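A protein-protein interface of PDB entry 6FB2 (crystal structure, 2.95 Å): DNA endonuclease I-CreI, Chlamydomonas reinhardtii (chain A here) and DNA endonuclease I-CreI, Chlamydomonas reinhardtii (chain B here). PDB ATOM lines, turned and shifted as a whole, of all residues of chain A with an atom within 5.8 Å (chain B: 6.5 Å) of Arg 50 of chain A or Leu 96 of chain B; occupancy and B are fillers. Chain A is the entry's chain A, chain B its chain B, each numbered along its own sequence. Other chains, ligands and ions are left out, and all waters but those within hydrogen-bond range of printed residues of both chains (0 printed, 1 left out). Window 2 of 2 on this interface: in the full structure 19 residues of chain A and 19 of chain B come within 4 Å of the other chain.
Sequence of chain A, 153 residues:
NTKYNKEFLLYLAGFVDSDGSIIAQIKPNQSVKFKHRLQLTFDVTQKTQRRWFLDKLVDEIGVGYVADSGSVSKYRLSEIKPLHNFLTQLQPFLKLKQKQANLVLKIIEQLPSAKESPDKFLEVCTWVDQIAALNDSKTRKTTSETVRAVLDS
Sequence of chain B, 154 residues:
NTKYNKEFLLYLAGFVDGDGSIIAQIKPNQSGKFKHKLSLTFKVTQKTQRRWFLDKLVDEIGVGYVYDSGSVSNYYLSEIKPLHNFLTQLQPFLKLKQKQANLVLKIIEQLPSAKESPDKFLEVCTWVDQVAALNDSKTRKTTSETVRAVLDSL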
ATOM      1  N   TYR A  11       3.533  18.787  34.672  1.00  0.00           N
ATOM      2  CA  TYR A  11       3.315  18.700  33.232  1.00  0.00           C
ATOM      3  C   TYR A  11       2.419  19.833  32.753  1.00  0.00           C
ATOM      4  O   TYR A  11       2.738  20.517  31.781  1.00  0.00           O
ATOM      5  CB  TYR A  11       2.682  17.356  32.855  1.00  0.00           C
ATOM      6  CG  TYR A  11       2.270  17.267  31.399  1.00  0.00           C
ATOM      7  CD1 TYR A  11       1.011  17.687  30.983  1.00  0.00           C
ATOM      8  CD2 TYR A  11       3.139  16.765  30.442  1.00  0.00           C
ATOM      9  CE1 TYR A  11       0.637  17.617  29.662  1.00  0.00           C
ATOM     10  CE2 TYR A  11       2.768  16.685  29.115  1.00  0.00           C
ATOM     11  CZ  TYR A  11       1.518  17.115  28.734  1.00  0.00           C
ATOM     12  OH  TYR A  11       1.139  17.042  27.416  1.00  0.00           O
ATOM     13  N   PHE A  15       2.560  23.091  29.949  1.00  0.00           N
ATOM     14  CA  PHE A  15       1.614  23.221  28.850  1.00  0.00           C
ATOM     15  C   PHE A  15       0.952  24.595  28.874  1.00  0.00           C
ATOM     16  O   PHE A  15       0.721  25.199  27.825  1.00  0.00           O
ATOM     17  CB  PHE A  15       0.554  22.122  28.932  1.00  0.00           C
ATOM     18  CG  PHE A  15      -0.158  21.869  27.634  1.00  0.00           C
ATOM     19  CD1 PHE A  15      -1.201  22.686  27.225  1.00  0.00           C
ATOM     20  CD2 PHE A  15       0.210  20.806  26.827  1.00  0.00           C
ATOM     21  CE1 PHE A  15      -1.854  22.450  26.031  1.00  0.00           C
ATOM     22  CE2 PHE A  15      -0.440  20.567  25.634  1.00  0.00           C
ATOM     23  CZ  PHE A  15      -1.473  21.391  25.237  1.00  0.00           C
ATOM     24  N   GLN A  46      -6.239  24.610  21.899  1.00  0.00           N
ATOM     25  CA  GLN A  46      -5.729  23.517  21.075  1.00  0.00           C
ATOM     26  C   GLN A  46      -6.674  23.314  19.895  1.00  0.00           C
ATOM     27  O   GLN A  46      -7.875  23.550  20.018  1.00  0.00           O
ATOM     28  CB  GLN A  46      -5.628  22.231  21.896  1.00  0.00           C
ATOM     29  CG  GLN A  46      -4.623  21.222  21.359  1.00  0.00           C
ATOM     30  CD  GLN A  46      -3.191  21.664  21.567  1.00  0.00           C
ATOM     31  OE1 GLN A  46      -2.297  21.290  20.811  1.00  0.00           O
ATOM     32  NE2 GLN A  46      -2.963  22.463  22.602  1.00  0.00           N
ATOM     33  N   LYS A  47      -6.145  22.883  18.753  1.00  0.00           N
ATOM     34  CA  LYS A  47      -6.997  22.669  17.585  1.00  0.00           C
ATOM     35  C   LYS A  47      -7.920  21.469  17.788  1.00  0.00           C
ATOM     36  O   LYS A  47      -7.534  20.481  18.412  1.00  0.00           O
ATOM     37  CB  LYS A  47      -6.179  22.545  16.291  1.00  0.00           C
ATOM     38  CG  LYS A  47      -5.378  21.261  16.115  1.00  0.00           C
ATOM     39  CD  LYS A  47      -4.749  21.233  14.721  1.00  0.00           C
ATOM     40  CE  LYS A  47      -4.181  19.868  14.357  1.00  0.00           C
ATOM     41  NZ  LYS A  47      -2.882  19.592  15.020  1.00  0.00           N
ATOM     42  N   THR A  48      -9.140  21.578  17.263  1.00  0.00           N
ATOM     43  CA  THR A  48     -10.210  20.601  17.486  1.00  0.00           C
ATOM     44  C   THR A  48      -9.807  19.157  17.182  1.00  0.00           C
ATOM     45  O   THR A  48     -10.375  18.213  17.737  1.00  0.00           O
ATOM     46  CB  THR A  48     -11.463  20.967  16.662  1.00  0.00           C
ATOM     47  OG1 THR A  48     -11.673  22.383  16.714  1.00  0.00           O
ATOM     48  CG2 THR A  48     -12.695  20.259  17.205  1.00  0.00           C
ATOM     49  N   GLN A  49      -8.817  18.994  16.311  1.00  0.00           N
ATOM     50  CA  GLN A  49      -8.264  17.683  15.994  1.00  0.00           C
ATOM     51  C   GLN A  49      -7.680  17.028  17.248  1.00  0.00           C
ATOM     52  O   GLN A  49      -7.495  15.812  17.298  1.00  0.00           O
ATOM     53  CB  GLN A  49      -7.193  17.827  14.908  1.00  0.00           C
ATOM     54  CG  GLN A  49      -6.615  16.519  14.388  1.00  0.00           C
ATOM     55  CD  GLN A  49      -5.587  16.736  13.291  1.00  0.00           C
ATOM     56  OE1 GLN A  49      -5.846  17.434  12.310  1.00  0.00           O
ATOM     57  NE2 GLN A  49      -4.411  16.141  13.456  1.00  0.00           N
ATOM     58  N   ARG A  50      -7.400  17.844  18.261  1.00  0.00           N
ATOM     59  CA  ARG A  50      -6.911  17.351  19.542  1.00  0.00           C
ATOM     60  C   ARG A  50      -7.804  17.802  20.692  1.00  0.00           C
ATOM     61  O   ARG A  50      -7.318  18.061  21.792  1.00  0.00           O
ATOM     62  CB  ARG A  50      -5.477  17.822  19.793  1.00  0.00           C
ATOM     63  CG  ARG A  50      -4.425  17.091  18.978  1.00  0.00           C
ATOM     64  CD  ARG A  50      -3.020  17.464  19.423  1.00  0.00           C
ATOM     65  NE  ARG A  50      -2.647  18.809  18.997  1.00  0.00           N
ATOM     66  CZ  ARG A  50      -1.914  19.066  17.921  1.00  0.00           C
ATOM     67  NH1 ARG A  50      -1.470  18.069  17.167  1.00  0.00           N
ATOM     68  NH2 ARG A  50      -1.619  20.317  17.598  1.00  0.00           N
ATOM     69  N   ARG A  51      -9.105  17.891  20.430  1.00  0.00           N
ATOM     70  CA  ARG A  51     -10.079  18.283  21.447  1.00  0.00           C
ATOM     71  C   ARG A  51     -10.056  17.321  22.634  1.00  0.00           C
ATOM     72  O   ARG A  51     -10.290  17.719  23.776  1.00  0.00           O
ATOM     73  CB  ARG A  51     -11.485  18.334  20.841  1.00  0.00           C
ATOM     74  CG  ARG A  51     -12.574  18.731  21.828  1.00  0.00           C
ATOM     75  CD  ARG A  51     -13.949  18.273  21.373  1.00  0.00           C
ATOM     76  NE  ARG A  51     -14.905  18.288  22.476  1.00  0.00           N
ATOM     77  CZ  ARG A  51     -15.736  19.292  22.733  1.00  0.00           C
ATOM     78  NH1 ARG A  51     -15.738  20.369  21.959  1.00  0.00           N
ATOM     79  NH2 ARG A  51     -16.567  19.218  23.763  1.00  0.00           N
ATOM     80  N   TRP A  52      -9.760  16.057  22.348  1.00  0.00           N
ATOM     81  CA  TRP A  52      -9.702  15.014  23.365  1.00  0.00           C
ATOM     82  C   TRP A  52      -8.744  15.345  24.505  1.00  0.00           C
ATOM     83  O   TRP A  52      -9.028  15.038  25.662  1.00  0.00           O
ATOM     84  CB  TRP A  52      -9.293  13.688  22.728  1.00  0.00           C
ATOM     85  CG  TRP A  52      -7.890  13.675  22.209  1.00  0.00           C
ATOM     86  CD1 TRP A  52      -7.466  14.082  20.979  1.00  0.00           C
ATOM     87  CD2 TRP A  52      -6.723  13.227  22.908  1.00  0.00           C
ATOM     88  NE1 TRP A  52      -6.107  13.918  20.868  1.00  0.00           N
ATOM     89  CE2 TRP A  52      -5.626  13.394  22.040  1.00  0.00           C
ATOM     90  CE3 TRP A  52      -6.498  12.703  24.183  1.00  0.00           C
ATOM     91  CZ2 TRP A  52      -4.327  13.056  22.407  1.00  0.00           C
ATOM     92  CZ3 TRP A  52      -5.209  12.367  24.544  1.00  0.00           C
ATOM     93  CH2 TRP A  52      -4.140  12.544  23.661  1.00  0.00           C
ATOM     94  N   PHE A  53      -7.613  15.959  24.172  1.00  0.00           N
ATOM     95  CA  PHE A  53      -6.620  16.318  25.175  1.00  0.00           C
ATOM     96  C   PHE A  53      -7.190  17.359  26.127  1.00  0.00           C
ATOM     97  O   PHE A  53      -6.811  17.418  27.296  1.00  0.00           O
ATOM     98  CB  PHE A  53      -5.346  16.845  24.508  1.00  0.00           C
ATOM     99  CG  PHE A  53      -4.288  17.285  25.482  1.00  0.00           C
ATOM    100  CD1 PHE A  53      -3.368  16.379  25.985  1.00  0.00           C
ATOM    101  CD2 PHE A  53      -4.210  18.608  25.892  1.00  0.00           C
ATOM    102  CE1 PHE A  53      -2.395  16.782  26.880  1.00  0.00           C
ATOM    103  CE2 PHE A  53      -3.243  19.013  26.788  1.00  0.00           C
ATOM    104  CZ  PHE A  53      -2.332  18.101  27.280  1.00  0.00           C
ATOM    105  N   LEU A  54      -8.101  18.181  25.617  1.00  0.00           N
ATOM    106  CA  LEU A  54      -8.767  19.187  26.432  1.00  0.00           C
ATOM    107  C   LEU A  54      -9.889  18.556  27.254  1.00  0.00           C
ATOM    108  O   LEU A  54     -10.244  19.060  28.320  1.00  0.00           O
ATOM    109  CB  LEU A  54      -9.321  20.310  25.553  1.00  0.00           C
ATOM    110  CG  LEU A  54      -8.294  21.157  24.798  1.00  0.00           C
ATOM    111  CD1 LEU A  54      -8.973  22.170  23.894  1.00  0.00           C
ATOM    112  CD2 LEU A  54      -7.369  21.859  25.772  1.00  0.00           C
ATOM    113  N   ASP B  17       4.947  19.608  24.255  1.00  0.00           N
ATOM    114  CA  ASP B  17       3.643  19.326  23.671  1.00  0.00           C
ATOM    115  C   ASP B  17       2.904  20.624  23.346  1.00  0.00           C
ATOM    116  O   ASP B  17       2.053  20.658  22.456  1.00  0.00           O
ATOM    117  CB  ASP B  17       2.809  18.461  24.617  1.00  0.00           C
ATOM    118  CG  ASP B  17       3.284  17.021  24.662  1.00  0.00           C
ATOM    119  OD1 ASP B  17       3.785  16.524  23.633  1.00  0.00           O
ATOM    120  OD2 ASP B  17       3.149  16.381  25.725  1.00  0.00           O
ATOM    121  N   GLY B  18       3.242  21.690  24.067  1.00  0.00           N
ATOM    122  CA  GLY B  18       2.655  22.996  23.826  1.00  0.00           C
ATOM    123  C   GLY B  18       3.318  23.752  22.687  1.00  0.00           C
ATOM    124  O   GLY B  18       2.746  23.882  21.605  1.00  0.00           O
ATOM    125  N   PHE B  93       7.061  11.133  29.321  1.00  0.00           N
ATOM    126  CA  PHE B  93       6.197  12.172  29.875  1.00  0.00           C
ATOM    127  C   PHE B  93       5.440  12.944  28.796  1.00  0.00           C
ATOM    128  O   PHE B  93       4.504  13.688  29.095  1.00  0.00           O
ATOM    129  CB  PHE B  93       7.013  13.132  30.739  1.00  0.00           C
ATOM    130  CG  PHE B  93       7.873  12.443  31.755  1.00  0.00           C
ATOM    131  CD1 PHE B  93       7.318  11.923  32.912  1.00  0.00           C
ATOM    132  CD2 PHE B  93       9.235  12.317  31.553  1.00  0.00           C
ATOM    133  CE1 PHE B  93       8.108  11.288  33.848  1.00  0.00           C
ATOM    134  CE2 PHE B  93      10.031  11.684  32.486  1.00  0.00           C
ATOM    135  CZ  PHE B  93       9.466  11.169  33.634  1.00  0.00           C
ATOM    136  N   LEU B  94       5.851  12.767  27.545  1.00  0.00           N
ATOM    137  CA  LEU B  94       5.158  13.391  26.425  1.00  0.00           C
ATOM    138  C   LEU B  94       3.788  12.751  26.222  1.00  0.00           C
ATOM    139  O   LEU B  94       3.612  11.554  26.454  1.00  0.00           O
ATOM    140  CB  LEU B  94       5.990  13.274  25.146  1.00  0.00           C
ATOM    141  CG  LEU B  94       7.302  14.061  25.108  1.00  0.00           C
ATOM    142  CD1 LEU B  94       8.089  13.759  23.843  1.00  0.00           C
ATOM    143  CD2 LEU B  94       7.026  15.548  25.214  1.00  0.00           C
ATOM    144  N   LYS B  95       2.820  13.555  25.799  1.00  0.00           N
ATOM    145  CA  LYS B  95       1.482  13.054  25.513  1.00  0.00           C
ATOM    146  C   LYS B  95       1.129  13.302  24.053  1.00  0.00           C
ATOM    147  O   LYS B  95       0.714  12.390  23.340  1.00  0.00           O
ATOM    148  CB  LYS B  95       0.451  13.716  26.431  1.00  0.00           C
ATOM    149  CG  LYS B  95       0.592  13.332  27.897  1.00  0.00           C
ATOM    150  CD  LYS B  95      -0.416  14.062  28.774  1.00  0.00           C
ATOM    151  CE  LYS B  95      -0.374  13.545  30.204  1.00  0.00           C
ATOM    152  NZ  LYS B  95       1.001  13.580  30.769  1.00  0.00           N
ATOM    153  N   LEU B  96       1.314  14.541  23.609  1.00  0.00           N
ATOM    154  CA  LEU B  96       0.951  14.932  22.250  1.00  0.00           C
ATOM    155  C   LEU B  96       2.015  14.565  21.218  1.00  0.00           C
ATOM    156  O   LEU B  96       1.712  14.408  20.035  1.00  0.00           O
ATOM    157  CB  LEU B  96       0.663  16.434  22.186  1.00  0.00           C
ATOM    158  CG  LEU B  96      -0.562  16.927  22.955  1.00  0.00           C
ATOM    159  CD1 LEU B  96      -0.867  18.378  22.631  1.00  0.00           C
ATOM    160  CD2 LEU B  96      -1.755  16.054  22.645  1.00  0.00           C
ATOM    161  N   LYS B  97       3.259  14.422  21.666  1.00  0.00           N
ATOM    162  CA  LYS B  97       4.373  14.205  20.752  1.00  0.00           C
ATOM    163  C   LYS B  97       5.252  13.026  21.158  1.00  0.00           C
ATOM    164  O   LYS B  97       6.467  13.057  20.964  1.00  0.00           O
ATOM    165  CB  LYS B  97       5.211  15.482  20.644  1.00  0.00           C
ATOM    166  CG  LYS B  97       4.496  16.626  19.941  1.00  0.00           C
ATOM    167  CD  LYS B  97       5.112  17.973  20.275  1.00  0.00           C
ATOM    168  CE  LYS B  97       4.454  19.081  19.469  1.00  0.00           C
ATOM    169  NZ  LYS B  97       4.693  18.902  18.012  1.00  0.00           N
ATOM    170  N   GLN B  98       4.639  11.981  21.705  1.00  0.00           N
ATOM    171  CA  GLN B  98       5.387  10.811  22.152  1.00  0.00           C
ATOM    172  C   GLN B  98       5.737   9.881  20.989  1.00  0.00           C
ATOM    173  O   GLN B  98       6.825   9.306  20.952  1.00  0.00           O
ATOM    174  CB  GLN B  98       4.607  10.049  23.226  1.00  0.00           C
ATOM    175  CG  GLN B  98       5.399   8.930  23.884  1.00  0.00           C
ATOM    176  CD  GLN B  98       4.657   8.282  25.034  1.00  0.00           C
ATOM    177  OE1 GLN B  98       3.476   7.954  24.921  1.00  0.00           O
ATOM    178  NE2 GLN B  98       5.348   8.098  26.153  1.00  0.00           N
ATOM    179  N   LYS B  99       4.809   9.740  20.046  1.00  0.00           N
ATOM    180  CA  LYS B  99       5.034   8.914  18.863  1.00  0.00           C
ATOM    181  C   LYS B  99       6.192   9.449  18.027  1.00  0.00           C
ATOM    182  O   LYS B  99       6.971   8.679  17.467  1.00  0.00           O
ATOM    183  CB  LYS B  99       3.770   8.848  18.004  1.00  0.00           C
ATOM    184  CG  LYS B  99       2.701   7.882  18.504  1.00  0.00           C
ATOM    185  CD  LYS B  99       1.461   7.950  17.620  1.00  0.00           C
ATOM    186  CE  LYS B  99       0.418   6.918  18.021  1.00  0.00           C
ATOM    187  NZ  LYS B  99      -0.843   7.079  17.240  1.00  0.00           N
ATOM    188  N   GLN B 100       6.295  10.773  17.944  1.00  0.00           N
ATOM    189  CA  GLN B 100       7.362  11.414  17.185  1.00  0.00           C
ATOM    190  C   GLN B 100       8.725  11.165  17.824  1.00  0.00           C
ATOM    191  O   GLN B 100       9.725  10.999  17.127  1.00  0.00           O
ATOM    192  CB  GLN B 100       7.108  12.920  17.061  1.00  0.00           C
ATOM    193  CG  GLN B 100       5.886  13.298  16.226  1.00  0.00           C
ATOM    194  CD  GLN B 100       4.593  13.272  17.017  1.00  0.00           C
ATOM    195  OE1 GLN B 100       4.413  12.446  17.912  1.00  0.00           O
ATOM    196  NE2 GLN B 100       3.683  14.183  16.692  1.00  0.00           N
ATOM    197  N   LEU B 134       2.477  12.893  11.659  1.00  0.00           N
ATOM    198  CA  LEU B 134       2.024  13.169  13.017  1.00  0.00           C
ATOM    199  C   LEU B 134       2.061  14.667  13.305  1.00  0.00           C
ATOM    200  O   LEU B 134       1.161  15.209  13.951  1.00  0.00           O
ATOM    201  CB  LEU B 134       2.893  12.413  14.022  1.00  0.00           C
ATOM    202  CG  LEU B 134       2.754  10.891  14.011  1.00  0.00           C
ATOM    203  CD1 LEU B 134       3.983  10.231  14.606  1.00  0.00           C
ATOM    204  CD2 LEU B 134       1.512  10.468  14.771  1.00  0.00           C
ATOM    205  N   ASN B 135       3.106  15.331  12.823  1.00  0.00           N
ATOM    206  CA  ASN B 135       3.216  16.776  12.960  1.00  0.00           C
ATOM    207  C   ASN B 135       2.187  17.483  12.086  1.00  0.00           C
ATOM    208  O   ASN B 135       1.651  16.893  11.146  1.00  0.00           O
ATOM    209  CB  ASN B 135       4.622  17.246  12.586  1.00  0.00           C
ATOM    210  CG  ASN B 135       5.688  16.692  13.509  1.00  0.00           C
ATOM    211  OD1 ASN B 135       5.394  16.235  14.612  1.00  0.00           O
ATOM    212  ND2 ASN B 135       6.937  16.741  13.066  1.00  0.00           N
ATOM    213  N   ASP B 136       1.913  18.745  12.397  1.00  0.00           N
ATOM    214  CA  ASP B 136       1.021  19.552  11.577  1.00  0.00           C
ATOM    215  C   ASP B 136       1.781  20.025  10.343  1.00  0.00           C
ATOM    216  O   ASP B 136       1.996  21.222  10.160  1.00  0.00           O
ATOM    217  CB  ASP B 136       0.508  20.754  12.371  1.00  0.00           C
ATOM    218  CG  ASP B 136       0.031  20.376  13.762  1.00  0.00           C
ATOM    219  OD1 ASP B 136      -0.350  19.205  13.966  1.00  0.00           O
ATOM    220  OD2 ASP B 136       0.036  21.253  14.652  1.00  0.00           O
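Of the 11 printed residues of chain A, 7 touch a printed residue of chain B.
Hydrophobic or aromatic side chains of chain A within 4 Å of the printed part of chain B: Tyr 11, Phe 15, Trp 52 and Phe 53.
Among the printed residues, Asp or Glu carboxylates within 4 Å of a Lys or Arg side-chain nitrogen of the other chain: Lys 47 of chain A with Asp 136 of chain B (2.8 Å) and Arg 50 of chain A with Asp 136 of chain B (3.5 Å).
The side-chain carboxylate (OD2) of Asp 17 of chain B is in hydrogen-bond range of the backbone NH (N) of Lys 95 of chain B, at 2.8 Å.
NE of Arg 50 of chain A sits at hydrogen-bond distance from OE1 of Gln 46 of chain A (3.1 Å).
The backbone NH (N) of Leu 96 of chain B lies within hydrogen-bond range of the side-chain carboxylate (OD1) of Asp 17 of chain B.
OD1 of Asp 17 of chain B is in hydrogen-bond range of N of Lys 97 of chain B, 2.9 Å away.
O of Phe 93 of chain B touches CE2 of Tyr 11 of chain A, at 3.5 Å.
Tyr 11 of chain A touches Lys 95 of chain B.
CD1 of Leu 96 of chain B touches CE2 of Phe 15 of chain A (3.7 Å).
OE1 of Gln 46 of chain A touches CD1 of Leu 96 of chain B, at 3.7 Å.
Arg 50 of chain A touches Leu 96 of chain B.
Leu 96 of chain B touches Trp 52 of chain A (CD2 to CZ2, 3.96 Å).
CE1 of Phe 53 of chain A touches CD of Lys 95 of chain B (3.9 Å).
CD1 of Phe 53 of chain A touches CD2 of Leu 96 of chain B, 3.7 Å away.
Of the printed residues of chain B, Phe 15 of chain A touches Leu 96.
Printed residues of chain B within 4 Å of Gln 46 of chain A: Leu 96 (3.7 Å).
Of the printed residues of chain B, Arg 50 of chain A touches Leu 96 (3.7 Å) and Asp 136 (3.5 Å).
Printed residues of chain A within 4 Å of Asp 17 of chain B: Tyr 11.
Of the printed residues of chain A, Lys 95 of chain B touches Tyr 11 (3.5 Å) and Phe 53 (3.9 Å).
The nearest residue of chain A that does not touch Leu 96 of chain B is Tyr 11 of chain A (4.6 Å).
The nearest printed residue of chain B that does not touch Phe 53 of chain A is Asp 17 of chain B (5.7 Å).
OD1 of Asp 136 of chain B is in salt-bridge range of NZ of Lys 47 of chain A (2.8 Å).
NH2 of Arg 50 of chain A lies within salt-bridge range of OD2 of Asp 136 of chain B.
The side-chain carboxylate (OD2) of Asp 17 of chain B lies within hydrogen-bond range of the side-chain hydroxyl (OH) of Tyr 11 of chain A (2.7 Å).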
